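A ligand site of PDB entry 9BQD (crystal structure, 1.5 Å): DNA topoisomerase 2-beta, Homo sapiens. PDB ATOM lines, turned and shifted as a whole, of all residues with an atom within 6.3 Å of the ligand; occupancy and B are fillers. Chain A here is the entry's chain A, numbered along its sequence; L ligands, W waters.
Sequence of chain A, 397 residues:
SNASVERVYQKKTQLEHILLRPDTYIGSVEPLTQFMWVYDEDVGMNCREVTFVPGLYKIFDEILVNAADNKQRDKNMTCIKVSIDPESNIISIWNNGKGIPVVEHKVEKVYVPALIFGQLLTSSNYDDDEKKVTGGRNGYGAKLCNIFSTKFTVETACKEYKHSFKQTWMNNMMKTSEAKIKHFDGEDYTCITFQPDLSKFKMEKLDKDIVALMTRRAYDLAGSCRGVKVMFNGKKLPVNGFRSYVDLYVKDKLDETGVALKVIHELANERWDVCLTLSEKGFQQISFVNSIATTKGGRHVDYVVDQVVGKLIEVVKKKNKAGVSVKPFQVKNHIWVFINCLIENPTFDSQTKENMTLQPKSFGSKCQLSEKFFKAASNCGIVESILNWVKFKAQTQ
NH1 of Arg 216 sits at hydrogen-bond distance from O of Trp 37. OE1 of Gln 285 sits at hydrogen-bond distance from OG of Ser 287, at 2.6 Å. The side-chain carboxylate of Glu 354 lies within hydrogen-bond range of the side-chain hydroxyl of Thr 295 (2.6 Å). The backbone carbonyl oxygen of Met 36 lies close to the side-chain sulfur of Cys 47 (3.7 Å). OD2 of Asp 220 is in salt-bridge range of NH1 of Arg 217 (3.0 Å). The backbone NH (N) of Lys 296 lies within hydrogen-bond range of the backbone carbonyl oxygen (O) of Glu 354 (2.8 Å). The backbone carbonyl oxygen of Glu 354 sits at hydrogen-bond distance from the backbone NH of Gly 297, 3.3 Å away. The backbone NH (N) of Leu 32 sits at hydrogen-bond distance from the backbone carbonyl oxygen (O) of Phe 52.
Gln 34 touches the ligand. Phe 35 touches the ligand. CE of Met 36 touches O2 of the ligand (3.7 Å). Phe 52 touches the ligand. Leu 213 touches the ligand (CD1 to O4, 3.6 Å). Asp 220 touches the ligand. OH of Tyr 245 touches C25 of the ligand, at 3.6 Å. Tyr 249 touches the ligand (OH to C25, 3.3 Å). Gln 284 touches the ligand. O of Gln 285 touches C27 of the ligand (3.2 Å). Ile 286 touches the ligand (CA to C22, 3.8 Å). Ser 287 touches the ligand (O to C16, 3.5 Å). Phe 288 touches the ligand. Ala 293 touches the ligand. O of Thr 294 touches C22 of the ligand, 3.5 Å away. Thr 295 touches the ligand. Glu 354 touches the ligand (OE1 to C17, 3.9 Å). Hydrophobic or aromatic side chains that line the ligand: Met 36, Trp 37, Phe 52, Tyr 57, Leu 213, Ile 286, Phe 288 and Ala 293. Within 4 Å of the ligand: Gln 34, Phe 35, Met 36, Trp 37, Phe 52, Tyr 57, Leu 213, Arg 216, Asp 220, Tyr 245, Tyr 249, Gln 284, Gln 285, Ile 286, Ser 287, Phe 288, Ala 293, Thr 294, Thr 295 and Glu 354. The nearest printed residue that does not touch the ligand is Arg 217 (4.1 Å).
The guanidinium group (NH2) of Arg 216 sits at hydrogen-bond distance from an oxygen (O4) of the ligand (2.9 Å). An oxygen (O3) of the ligand is in hydrogen-bond range of the backbone NH of Trp 37. An oxygen (O4) of the ligand sits at hydrogen-bond distance from the side-chain hydroxyl (OH) of Tyr 57.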
ATOM      1  N   LEU A  32      19.016  14.446 -10.450  1.00  0.00           N
ATOM      2  CA  LEU A  32      18.783  14.254  -9.024  1.00  0.00           C
ATOM      3  C   LEU A  32      18.113  15.529  -8.535  1.00  0.00           C
ATOM      4  O   LEU A  32      18.503  16.623  -8.965  1.00  0.00           O
ATOM      5  CB  LEU A  32      20.130  14.111  -8.321  1.00  0.00           C
ATOM      6  CG  LEU A  32      20.161  14.006  -6.802  1.00  0.00           C
ATOM      7  CD1 LEU A  32      19.280  12.859  -6.316  1.00  0.00           C
ATOM      8  CD2 LEU A  32      21.601  13.784  -6.332  1.00  0.00           C
ATOM      9  N   GLN A  34      17.406  17.438  -4.887  1.00  0.00           N
ATOM     10  CA  GLN A  34      17.588  17.424  -3.446  1.00  0.00           C
ATOM     11  C   GLN A  34      17.738  18.838  -2.928  1.00  0.00           C
ATOM     12  O   GLN A  34      18.033  19.775  -3.666  1.00  0.00           O
ATOM     13  CB  GLN A  34      18.785  16.556  -3.034  1.00  0.00           C
ATOM     14  CG  GLN A  34      20.125  17.162  -3.364  1.00  0.00           C
ATOM     15  CD  GLN A  34      21.306  16.333  -2.868  1.00  0.00           C
ATOM     16  OE1 GLN A  34      21.431  16.032  -1.675  1.00  0.00           O
ATOM     17  NE2 GLN A  34      22.190  15.990  -3.764  1.00  0.00           N
ATOM     18  N   PHE A  35      17.511  18.968  -1.629  1.00  0.00           N
ATOM     19  CA  PHE A  35      17.749  20.234  -0.942  1.00  0.00           C
ATOM     20  C   PHE A  35      19.229  20.412  -0.734  1.00  0.00           C
ATOM     21  O   PHE A  35      19.912  19.542  -0.200  1.00  0.00           O
ATOM     22  CB  PHE A  35      17.077  20.225   0.426  1.00  0.00           C
ATOM     23  CG  PHE A  35      15.647  20.577   0.386  1.00  0.00           C
ATOM     24  CD1 PHE A  35      15.236  21.895   0.424  1.00  0.00           C
ATOM     25  CD2 PHE A  35      14.679  19.577   0.315  1.00  0.00           C
ATOM     26  CE1 PHE A  35      13.890  22.219   0.404  1.00  0.00           C
ATOM     27  CE2 PHE A  35      13.335  19.893   0.289  1.00  0.00           C
ATOM     28  CZ  PHE A  35      12.937  21.212   0.328  1.00  0.00           C
ATOM     29  N   MET A  36      19.720  21.567  -1.129  1.00  0.00           N
ATOM     30  CA  MET A  36      21.127  21.868  -0.902  1.00  0.00           C
ATOM     31  C   MET A  36      21.315  23.366  -1.028  1.00  0.00           C
ATOM     32  O   MET A  36      20.385  24.099  -1.390  1.00  0.00           O
ATOM     33  CB  MET A  36      22.004  21.147  -1.901  1.00  0.00           C
ATOM     34  CG  MET A  36      21.629  21.512  -3.306  1.00  0.00           C
ATOM     35  SD  MET A  36      22.345  20.405  -4.511  1.00  0.00           S
ATOM     36  CE  MET A  36      23.966  20.987  -4.221  1.00  0.00           C
ATOM     37  N   TRP A  37      22.525  23.808  -0.735  1.00  0.00           N
ATOM     38  CA  TRP A  37      22.885  25.218  -0.826  1.00  0.00           C
ATOM     39  C   TRP A  37      23.394  25.524  -2.218  1.00  0.00           C
ATOM     40  O   TRP A  37      24.235  24.797  -2.749  1.00  0.00           O
ATOM     41  CB  TRP A  37      23.974  25.554   0.203  1.00  0.00           C
ATOM     42  CG  TRP A  37      23.559  25.343   1.610  1.00  0.00           C
ATOM     43  CD1 TRP A  37      23.742  24.212   2.376  1.00  0.00           C
ATOM     44  CD2 TRP A  37      22.895  26.290   2.442  1.00  0.00           C
ATOM     45  NE1 TRP A  37      23.230  24.415   3.626  1.00  0.00           N
ATOM     46  CE2 TRP A  37      22.691  25.671   3.702  1.00  0.00           C
ATOM     47  CE3 TRP A  37      22.452  27.592   2.257  1.00  0.00           C
ATOM     48  CZ2 TRP A  37      22.056  26.325   4.751  1.00  0.00           C
ATOM     49  CZ3 TRP A  37      21.816  28.246   3.306  1.00  0.00           C
ATOM     50  CH2 TRP A  37      21.623  27.614   4.533  1.00  0.00           C
ATOM     51  N   VAL A  38      22.901  26.614  -2.804  1.00  0.00           N
ATOM     52  CA  VAL A  38      23.396  27.117  -4.077  1.00  0.00           C
ATOM     53  C   VAL A  38      23.460  28.638  -3.998  1.00  0.00           C
ATOM     54  O   VAL A  38      22.943  29.249  -3.066  1.00  0.00           O
ATOM     55  CB  VAL A  38      22.555  26.656  -5.279  1.00  0.00           C
ATOM     56  CG1 VAL A  38      22.627  25.138  -5.468  1.00  0.00           C
ATOM     57  CG2 VAL A  38      21.104  27.137  -5.151  1.00  0.00           C
ATOM     58  N   CYS A  47      19.295  27.804   0.650  1.00  0.00           N
ATOM     59  CA  CYS A  47      19.062  26.369   0.671  1.00  0.00           C
ATOM     60  C   CYS A  47      17.679  26.126   0.079  1.00  0.00           C
ATOM     61  O   CYS A  47      16.667  26.662   0.564  1.00  0.00           O
ATOM     62  CB  CYS A  47      19.171  25.822   2.075  1.00  0.00           C
ATOM     63  SG  CYS A  47      19.311  24.023   2.127  1.00  0.00           S
ATOM     64  N   PHE A  52      19.694  18.700 -10.657  1.00  0.00           N
ATOM     65  CA  PHE A  52      20.960  18.781 -11.389  1.00  0.00           C
ATOM     66  C   PHE A  52      21.457  17.364 -11.648  1.00  0.00           C
ATOM     67  O   PHE A  52      20.995  16.400 -11.026  1.00  0.00           O
ATOM     68  CB  PHE A  52      22.011  19.587 -10.596  1.00  0.00           C
ATOM     69  CG  PHE A  52      22.535  18.869  -9.397  1.00  0.00           C
ATOM     70  CD1 PHE A  52      21.748  18.720  -8.276  1.00  0.00           C
ATOM     71  CD2 PHE A  52      23.822  18.328  -9.384  1.00  0.00           C
ATOM     72  CE1 PHE A  52      22.200  18.031  -7.170  1.00  0.00           C
ATOM     73  CE2 PHE A  52      24.287  17.649  -8.272  1.00  0.00           C
ATOM     74  CZ  PHE A  52      23.480  17.494  -7.165  1.00  0.00           C
ATOM     75  N   PRO A  54      24.569  15.035 -11.231  1.00  0.00           N
ATOM     76  CA  PRO A  54      25.826  15.016 -10.476  1.00  0.00           C
ATOM     77  C   PRO A  54      27.088  14.940 -11.319  1.00  0.00           C
ATOM     78  O   PRO A  54      28.077  15.628 -11.019  1.00  0.00           O
ATOM     79  CB  PRO A  54      25.641  13.785  -9.561  1.00  0.00           C
ATOM     80  CG  PRO A  54      24.162  13.757  -9.335  1.00  0.00           C
ATOM     81  CD  PRO A  54      23.578  14.094 -10.675  1.00  0.00           C
ATOM     82  N   TYR A  57      28.148  18.454 -12.538  1.00  0.00           N
ATOM     83  CA  TYR A  57      28.777  19.126 -11.420  1.00  0.00           C
ATOM     84  C   TYR A  57      30.211  18.621 -11.217  1.00  0.00           C
ATOM     85  O   TYR A  57      31.141  19.402 -11.053  1.00  0.00           O
ATOM     86  CB  TYR A  57      27.918  18.926 -10.158  1.00  0.00           C
ATOM     87  CG  TYR A  57      28.659  18.954  -8.820  1.00  0.00           C
ATOM     88  CD1 TYR A  57      29.201  20.122  -8.319  1.00  0.00           C
ATOM     89  CD2 TYR A  57      28.765  17.806  -8.059  1.00  0.00           C
ATOM     90  CE1 TYR A  57      29.888  20.130  -7.089  1.00  0.00           C
ATOM     91  CE2 TYR A  57      29.439  17.805  -6.836  1.00  0.00           C
ATOM     92  CZ  TYR A  57      29.983  18.964  -6.357  1.00  0.00           C
ATOM     93  OH  TYR A  57      30.656  18.955  -5.122  1.00  0.00           O
ATOM     94  N   LEU A 213      24.810  26.000  -8.651  1.00  0.00           N
ATOM     95  CA  LEU A 213      25.690  25.062  -7.943  1.00  0.00           C
ATOM     96  C   LEU A 213      27.159  25.293  -8.283  1.00  0.00           C
ATOM     97  O   LEU A 213      28.017  25.357  -7.389  1.00  0.00           O
ATOM     98  CB  LEU A 213      25.262  23.638  -8.268  1.00  0.00           C
ATOM     99  CG  LEU A 213      26.121  22.514  -7.699  1.00  0.00           C
ATOM    100  CD1 LEU A 213      26.375  22.646  -6.194  1.00  0.00           C
ATOM    101  CD2 LEU A 213      25.491  21.136  -8.019  1.00  0.00           C
ATOM    102  N   ARG A 216      28.246  28.388  -6.585  1.00  0.00           N
ATOM    103  CA  ARG A 216      28.518  28.210  -5.172  1.00  0.00           C
ATOM    104  C   ARG A 216      29.887  27.556  -4.952  1.00  0.00           C
ATOM    105  O   ARG A 216      30.597  27.909  -3.994  1.00  0.00           O
ATOM    106  CB  ARG A 216      27.415  27.412  -4.468  1.00  0.00           C
ATOM    107  CG  ARG A 216      27.413  27.666  -2.954  1.00  0.00           C
ATOM    108  CD  ARG A 216      27.095  26.424  -2.154  1.00  0.00           C
ATOM    109  NE  ARG A 216      28.170  25.451  -2.303  1.00  0.00           N
ATOM    110  CZ  ARG A 216      28.029  24.231  -2.805  1.00  0.00           C
ATOM    111  NH1 ARG A 216      26.828  23.730  -3.077  1.00  0.00           N
ATOM    112  NH2 ARG A 216      29.112  23.501  -3.051  1.00  0.00           N
ATOM    113  N   ARG A 217      30.270  26.601  -5.817  1.00  0.00           N
ATOM    114  CA  ARG A 217      31.612  26.017  -5.654  1.00  0.00           C
ATOM    115  C   ARG A 217      32.710  27.078  -5.748  1.00  0.00           C
ATOM    116  O   ARG A 217      33.729  26.973  -5.067  1.00  0.00           O
ATOM    117  CB  ARG A 217      31.858  24.894  -6.651  1.00  0.00           C
ATOM    118  CG  ARG A 217      31.168  23.579  -6.318  1.00  0.00           C
ATOM    119  CD  ARG A 217      31.711  22.859  -5.076  1.00  0.00           C
ATOM    120  NE  ARG A 217      33.080  22.404  -5.275  1.00  0.00           N
ATOM    121  CZ  ARG A 217      34.089  22.661  -4.452  1.00  0.00           C
ATOM    122  NH1 ARG A 217      33.929  23.400  -3.364  1.00  0.00           N
ATOM    123  NH2 ARG A 217      35.289  22.165  -4.727  1.00  0.00           N
ATOM    124  N   ASP A 220      32.775  28.589  -2.412  1.00  0.00           N
ATOM    125  CA  ASP A 220      33.449  27.644  -1.522  1.00  0.00           C
ATOM    126  C   ASP A 220      34.956  27.840  -1.597  1.00  0.00           C
ATOM    127  O   ASP A 220      35.645  27.839  -0.575  1.00  0.00           O
ATOM    128  CB  ASP A 220      33.180  26.196  -1.950  1.00  0.00           C
ATOM    129  CG  ASP A 220      31.719  25.738  -1.833  1.00  0.00           C
ATOM    130  OD1 ASP A 220      30.902  26.524  -1.296  1.00  0.00           O
ATOM    131  OD2 ASP A 220      31.450  24.599  -2.296  1.00  0.00           O
ATOM    132  N   TYR A 245      33.184  33.276   4.652  1.00  0.00           N
ATOM    133  CA  TYR A 245      32.401  32.293   3.916  1.00  0.00           C
ATOM    134  C   TYR A 245      31.279  31.728   4.795  1.00  0.00           C
ATOM    135  O   TYR A 245      30.115  31.660   4.375  1.00  0.00           O
ATOM    136  CB  TYR A 245      33.334  31.195   3.401  1.00  0.00           C
ATOM    137  CG  TYR A 245      32.615  30.030   2.793  1.00  0.00           C
ATOM    138  CD1 TYR A 245      32.121  30.083   1.500  1.00  0.00           C
ATOM    139  CD2 TYR A 245      32.375  28.883   3.532  1.00  0.00           C
ATOM    140  CE1 TYR A 245      31.434  29.036   0.954  1.00  0.00           C
ATOM    141  CE2 TYR A 245      31.688  27.812   2.987  1.00  0.00           C
ATOM    142  CZ  TYR A 245      31.228  27.887   1.702  1.00  0.00           C
ATOM    143  OH  TYR A 245      30.538  26.802   1.215  1.00  0.00           O
ATOM    144  N   TYR A 249      26.104  31.638   5.382  1.00  0.00           N
ATOM    145  CA  TYR A 249      25.105  30.701   5.856  1.00  0.00           C
ATOM    146  C   TYR A 249      24.414  31.177   7.116  1.00  0.00           C
ATOM    147  O   TYR A 249      23.205  30.981   7.278  1.00  0.00           O
ATOM    148  CB  TYR A 249      25.776  29.346   6.159  1.00  0.00           C
ATOM    149  CG  TYR A 249      26.348  28.684   4.926  1.00  0.00           C
ATOM    150  CD1 TYR A 249      25.566  27.853   4.161  1.00  0.00           C
ATOM    151  CD2 TYR A 249      27.652  28.904   4.522  1.00  0.00           C
ATOM    152  CE1 TYR A 249      26.070  27.225   3.049  1.00  0.00           C
ATOM    153  CE2 TYR A 249      28.157  28.292   3.386  1.00  0.00           C
ATOM    154  CZ  TYR A 249      27.359  27.453   2.649  1.00  0.00           C
ATOM    155  OH  TYR A 249      27.815  26.802   1.528  1.00  0.00           O
ATOM    156  N   LYS A 281      17.625  21.343  12.695  1.00  0.00           N
ATOM    157  CA  LYS A 281      17.189  20.511  11.580  1.00  0.00           C
ATOM    158  C   LYS A 281      17.933  19.183  11.558  1.00  0.00           C
ATOM    159  O   LYS A 281      18.070  18.567  10.497  1.00  0.00           O
ATOM    160  CB  LYS A 281      17.414  21.230  10.242  1.00  0.00           C
ATOM    161  CG  LYS A 281      16.541  22.441   9.981  1.00  0.00           C
ATOM    162  CD  LYS A 281      17.051  23.158   8.730  1.00  0.00           C
ATOM    163  CE  LYS A 281      15.956  23.919   7.999  1.00  0.00           C
ATOM    164  NZ  LYS A 281      16.411  24.363   6.644  1.00  0.00           N
ATOM    165  N   PHE A 283      21.608  16.956  12.612  1.00  0.00           N
ATOM    166  CA  PHE A 283      23.031  17.195  12.402  1.00  0.00           C
ATOM    167  C   PHE A 283      23.264  17.744  10.996  1.00  0.00           C
ATOM    168  O   PHE A 283      22.723  17.210  10.012  1.00  0.00           O
ATOM    169  CB  PHE A 283      23.823  15.914  12.555  1.00  0.00           C
ATOM    170  CG  PHE A 283      25.290  16.083  12.293  1.00  0.00           C
ATOM    171  CD1 PHE A 283      26.056  16.867  13.128  1.00  0.00           C
ATOM    172  CD2 PHE A 283      25.897  15.514  11.180  1.00  0.00           C
ATOM    173  CE1 PHE A 283      27.397  17.076  12.895  1.00  0.00           C
ATOM    174  CE2 PHE A 283      27.254  15.715  10.943  1.00  0.00           C
ATOM    175  CZ  PHE A 283      28.010  16.496  11.801  1.00  0.00           C
ATOM    176  N   GLN A 284      24.092  18.782  10.910  1.00  0.00           N
ATOM    177  CA  GLN A 284      24.489  19.375   9.649  1.00  0.00           C
ATOM    178  C   GLN A 284      26.000  19.624   9.677  1.00  0.00           C
ATOM    179  O   GLN A 284      26.543  20.094  10.686  1.00  0.00           O
ATOM    180  CB  GLN A 284      23.832  20.738   9.428  1.00  0.00           C
ATOM    181  CG  GLN A 284      22.357  20.708   9.324  1.00  0.00           C
ATOM    182  CD  GLN A 284      21.806  22.081   9.013  1.00  0.00           C
ATOM    183  OE1 GLN A 284      21.962  22.589   7.898  1.00  0.00           O
ATOM    184  NE2 GLN A 284      21.163  22.684  10.011  1.00  0.00           N
ATOM    185  N   GLN A 285      26.656  19.324   8.563  1.00  0.00           N
ATOM    186  CA  GLN A 285      28.077  19.643   8.414  1.00  0.00           C
ATOM    187  C   GLN A 285      28.300  20.213   7.029  1.00  0.00           C
ATOM    188  O   GLN A 285      27.712  19.758   6.045  1.00  0.00           O
ATOM    189  CB  GLN A 285      28.983  18.423   8.620  1.00  0.00           C
ATOM    190  CG  GLN A 285      28.795  17.298   7.629  1.00  0.00           C
ATOM    191  CD  GLN A 285      29.601  17.469   6.347  1.00  0.00           C
ATOM    192  OE1 GLN A 285      30.498  18.315   6.257  1.00  0.00           O
ATOM    193  NE2 GLN A 285      29.290  16.661   5.346  1.00  0.00           N
ATOM    194  N   ILE A 286      29.133  21.249   6.985  1.00  0.00           N
ATOM    195  CA  ILE A 286      29.687  21.794   5.749  1.00  0.00           C
ATOM    196  C   ILE A 286      31.197  21.702   5.935  1.00  0.00           C
ATOM    197  O   ILE A 286      31.747  22.264   6.878  1.00  0.00           O
ATOM    198  CB  ILE A 286      29.211  23.232   5.516  1.00  0.00           C
ATOM    199  CG1 ILE A 286      27.721  23.202   5.058  1.00  0.00           C
ATOM    200  CG2 ILE A 286      30.067  23.924   4.490  1.00  0.00           C
ATOM    201  CD1 ILE A 286      27.103  24.521   4.819  1.00  0.00           C
ATOM    202  N   SER A 287      31.854  20.950   5.060  1.00  0.00           N
ATOM    203  CA  SER A 287      33.277  20.658   5.247  1.00  0.00           C
ATOM    204  C   SER A 287      34.016  20.553   3.918  1.00  0.00           C
ATOM    205  O   SER A 287      33.442  20.179   2.885  1.00  0.00           O
ATOM    206  CB  SER A 287      33.486  19.370   6.056  1.00  0.00           C
ATOM    207  OG  SER A 287      32.941  18.236   5.391  1.00  0.00           O
ATOM    208  N   PHE A 288      35.299  20.886   3.983  1.00  0.00           N
ATOM    209  CA  PHE A 288      36.211  20.845   2.863  1.00  0.00           C
ATOM    210  C   PHE A 288      37.501  20.184   3.303  1.00  0.00           C
ATOM    211  O   PHE A 288      38.027  20.472   4.388  1.00  0.00           O
ATOM    212  CB  PHE A 288      36.516  22.261   2.385  1.00  0.00           C
ATOM    213  CG  PHE A 288      35.271  23.010   2.037  1.00  0.00           C
ATOM    214  CD1 PHE A 288      34.694  22.859   0.786  1.00  0.00           C
ATOM    215  CD2 PHE A 288      34.630  23.762   2.989  1.00  0.00           C
ATOM    216  CE1 PHE A 288      33.507  23.508   0.494  1.00  0.00           C
ATOM    217  CE2 PHE A 288      33.437  24.406   2.702  1.00  0.00           C
ATOM    218  CZ  PHE A 288      32.879  24.285   1.445  1.00  0.00           C
ATOM    219  N   ALA A 293      34.725  19.714  -1.574  1.00  0.00           N
ATOM    220  CA  ALA A 293      33.524  19.695  -0.723  1.00  0.00           C
ATOM    221  C   ALA A 293      33.196  18.237  -0.367  1.00  0.00           C
ATOM    222  O   ALA A 293      32.765  17.465  -1.223  1.00  0.00           O
ATOM    223  CB  ALA A 293      32.334  20.354  -1.440  1.00  0.00           C
ATOM    224  N   THR A 294      33.433  17.870   0.889  1.00  0.00           N
ATOM    225  CA  THR A 294      33.198  16.507   1.353  1.00  0.00           C
ATOM    226  C   THR A 294      31.742  16.412   1.798  1.00  0.00           C
ATOM    227  O   THR A 294      31.398  16.482   2.986  1.00  0.00           O
ATOM    228  CB  THR A 294      34.210  16.121   2.433  1.00  0.00           C
ATOM    229  OG1 THR A 294      34.347  17.176   3.393  1.00  0.00           O
ATOM    230  CG2 THR A 294      35.559  15.866   1.790  1.00  0.00           C
ATOM    231  N   THR A 295      30.858  16.289   0.806  1.00  0.00           N
ATOM    232  CA  THR A 295      29.417  16.400   0.990  1.00  0.00           C
ATOM    233  C   THR A 295      28.792  15.203   1.689  1.00  0.00           C
ATOM    234  O   THR A 295      27.632  15.291   2.122  1.00  0.00           O
ATOM    235  CB  THR A 295      28.766  16.692  -0.365  1.00  0.00           C
ATOM    236  OG1 THR A 295      29.270  15.787  -1.362  1.00  0.00           O
ATOM    237  CG2 THR A 295      29.103  18.090  -0.793  1.00  0.00           C
ATOM    238  N   LYS A 296      29.522  14.104   1.882  1.00  0.00           N
ATOM    239  CA  LYS A 296      29.075  13.030   2.753  1.00  0.00           C
ATOM    240  C   LYS A 296      29.914  12.945   4.022  1.00  0.00           C
ATOM    241  O   LYS A 296      29.751  12.005   4.805  1.00  0.00           O
ATOM    242  CB  LYS A 296      29.094  11.697   2.007  1.00  0.00           C
ATOM    243  CG  LYS A 296      28.024  11.590   0.942  1.00  0.00           C
ATOM    244  CD  LYS A 296      28.098  10.269   0.205  1.00  0.00           C
ATOM    245  CE  LYS A 296      27.028  10.185  -0.878  1.00  0.00           C
ATOM    246  NZ  LYS A 296      25.661  10.520  -0.344  1.00  0.00           N
ATOM    247  N   GLY A 297      30.803  13.905   4.217  1.00  0.00           N
ATOM    248  CA  GLY A 297      31.564  14.011   5.437  1.00  0.00           C
ATOM    249  C   GLY A 297      32.813  13.156   5.430  1.00  0.00           C
ATOM    250  O   GLY A 297      33.523  13.122   4.432  1.00  0.00           O
ATOM    251  N   GLU A 354      33.287  12.366  -2.048  1.00  0.00           N
ATOM    252  CA  GLU A 354      32.304  12.919  -1.121  1.00  0.00           C
ATOM    253  C   GLU A 354      32.571  12.529   0.324  1.00  0.00           C
ATOM    254  O   GLU A 354      32.114  13.219   1.234  1.00  0.00           O
ATOM    255  CB  GLU A 354      30.880  12.435  -1.458  1.00  0.00           C
ATOM    256  CG  GLU A 354      30.275  13.012  -2.710  1.00  0.00           C
ATOM    257  CD  GLU A 354      28.730  12.891  -2.757  1.00  0.00           C
ATOM    258  OE1 GLU A 354      27.985  13.608  -1.992  1.00  0.00           O
ATOM    259  OE2 GLU A 354      28.277  12.090  -3.573  1.00  0.00           O
HETATM  260  C1  LIG L   1      18.111  19.341   6.135  1.00  0.00           C
HETATM  261  C2  LIG L   1      21.148  20.816   4.994  1.00  0.00           C
HETATM  262  C3  LIG L   1      22.265  20.647   3.141  1.00  0.00           C
HETATM  263  C4  LIG L   1      25.444  20.252  -0.244  1.00  0.00           C
HETATM  264  C5  LIG L   1      27.829  21.128   1.363  1.00  0.00           C
HETATM  265  C6  LIG L   1      24.755  17.724  -1.162  1.00  0.00           C
HETATM  266  C7  LIG L   1      26.002  19.725  -1.391  1.00  0.00           C
HETATM  267  C8  LIG L   1      24.524  19.545   0.424  1.00  0.00           C
HETATM  268  C9  LIG L   1      25.679  18.446  -1.888  1.00  0.00           C
HETATM  269  C10 LIG L   1      29.207  21.334   1.214  1.00  0.00           C
HETATM  270  C11 LIG L   1      27.545  20.093  -3.267  1.00  0.00           C
HETATM  271  C12 LIG L   1      27.389  20.161   2.254  1.00  0.00           C
HETATM  272  C13 LIG L   1      22.854  19.660   2.119  1.00  0.00           C
HETATM  273  N1  LIG L   1      21.286  20.121   3.891  1.00  0.00           N
HETATM  274  C14 LIG L   1      25.832  21.672   0.043  1.00  0.00           C
HETATM  275  O1  LIG L   1      24.012  20.200   1.529  1.00  0.00           O
HETATM  276  C15 LIG L   1      27.200  18.747  -3.791  1.00  0.00           C
HETATM  277  C16 LIG L   1      30.147  20.548   1.847  1.00  0.00           C
HETATM  278  C17 LIG L   1      25.983  16.581  -3.651  1.00  0.00           C
HETATM  279  C18 LIG L   1      18.882  19.903   4.185  1.00  0.00           C
HETATM  280  C19 LIG L   1      27.367  23.392   0.815  1.00  0.00           C
HETATM  281  C20 LIG L   1      20.114  20.072   3.273  1.00  0.00           C
HETATM  282  C21 LIG L   1      26.570  16.245  -5.035  1.00  0.00           C
HETATM  283  C22 LIG L   1      29.691  19.542   2.702  1.00  0.00           C
HETATM  284  C23 LIG L   1      29.639  22.526   0.251  1.00  0.00           C
HETATM  285  C24 LIG L   1      26.082  14.891  -5.554  1.00  0.00           C
HETATM  286  C25 LIG L   1      28.799  23.736   0.775  1.00  0.00           C
HETATM  287  C26 LIG L   1      20.100  20.221   5.949  1.00  0.00           C
HETATM  288  C27 LIG L   1      28.316  19.335   2.909  1.00  0.00           C
HETATM  289  C28 LIG L   1      24.168  18.259  -0.012  1.00  0.00           C
HETATM  290  C29 LIG L   1      26.370  17.986  -3.154  1.00  0.00           C
HETATM  291  N2  LIG L   1      26.995  22.074   0.704  1.00  0.00           N
HETATM  292  N3  LIG L   1      19.185  19.471   5.368  1.00  0.00           N
HETATM  293  O2  LIG L   1      26.956  20.526  -2.107  1.00  0.00           O
HETATM  294  O3  LIG L   1      25.102  22.534  -0.430  1.00  0.00           O
HETATM  295  O4  LIG L   1      28.326  20.840  -3.814  1.00  0.00           O
HETATM  296  O   HOH W   1      16.223  18.085   8.534  1.00  0.00           O
HETATM  297  O   HOH W   2      25.499  16.901   2.812  1.00  0.00           O
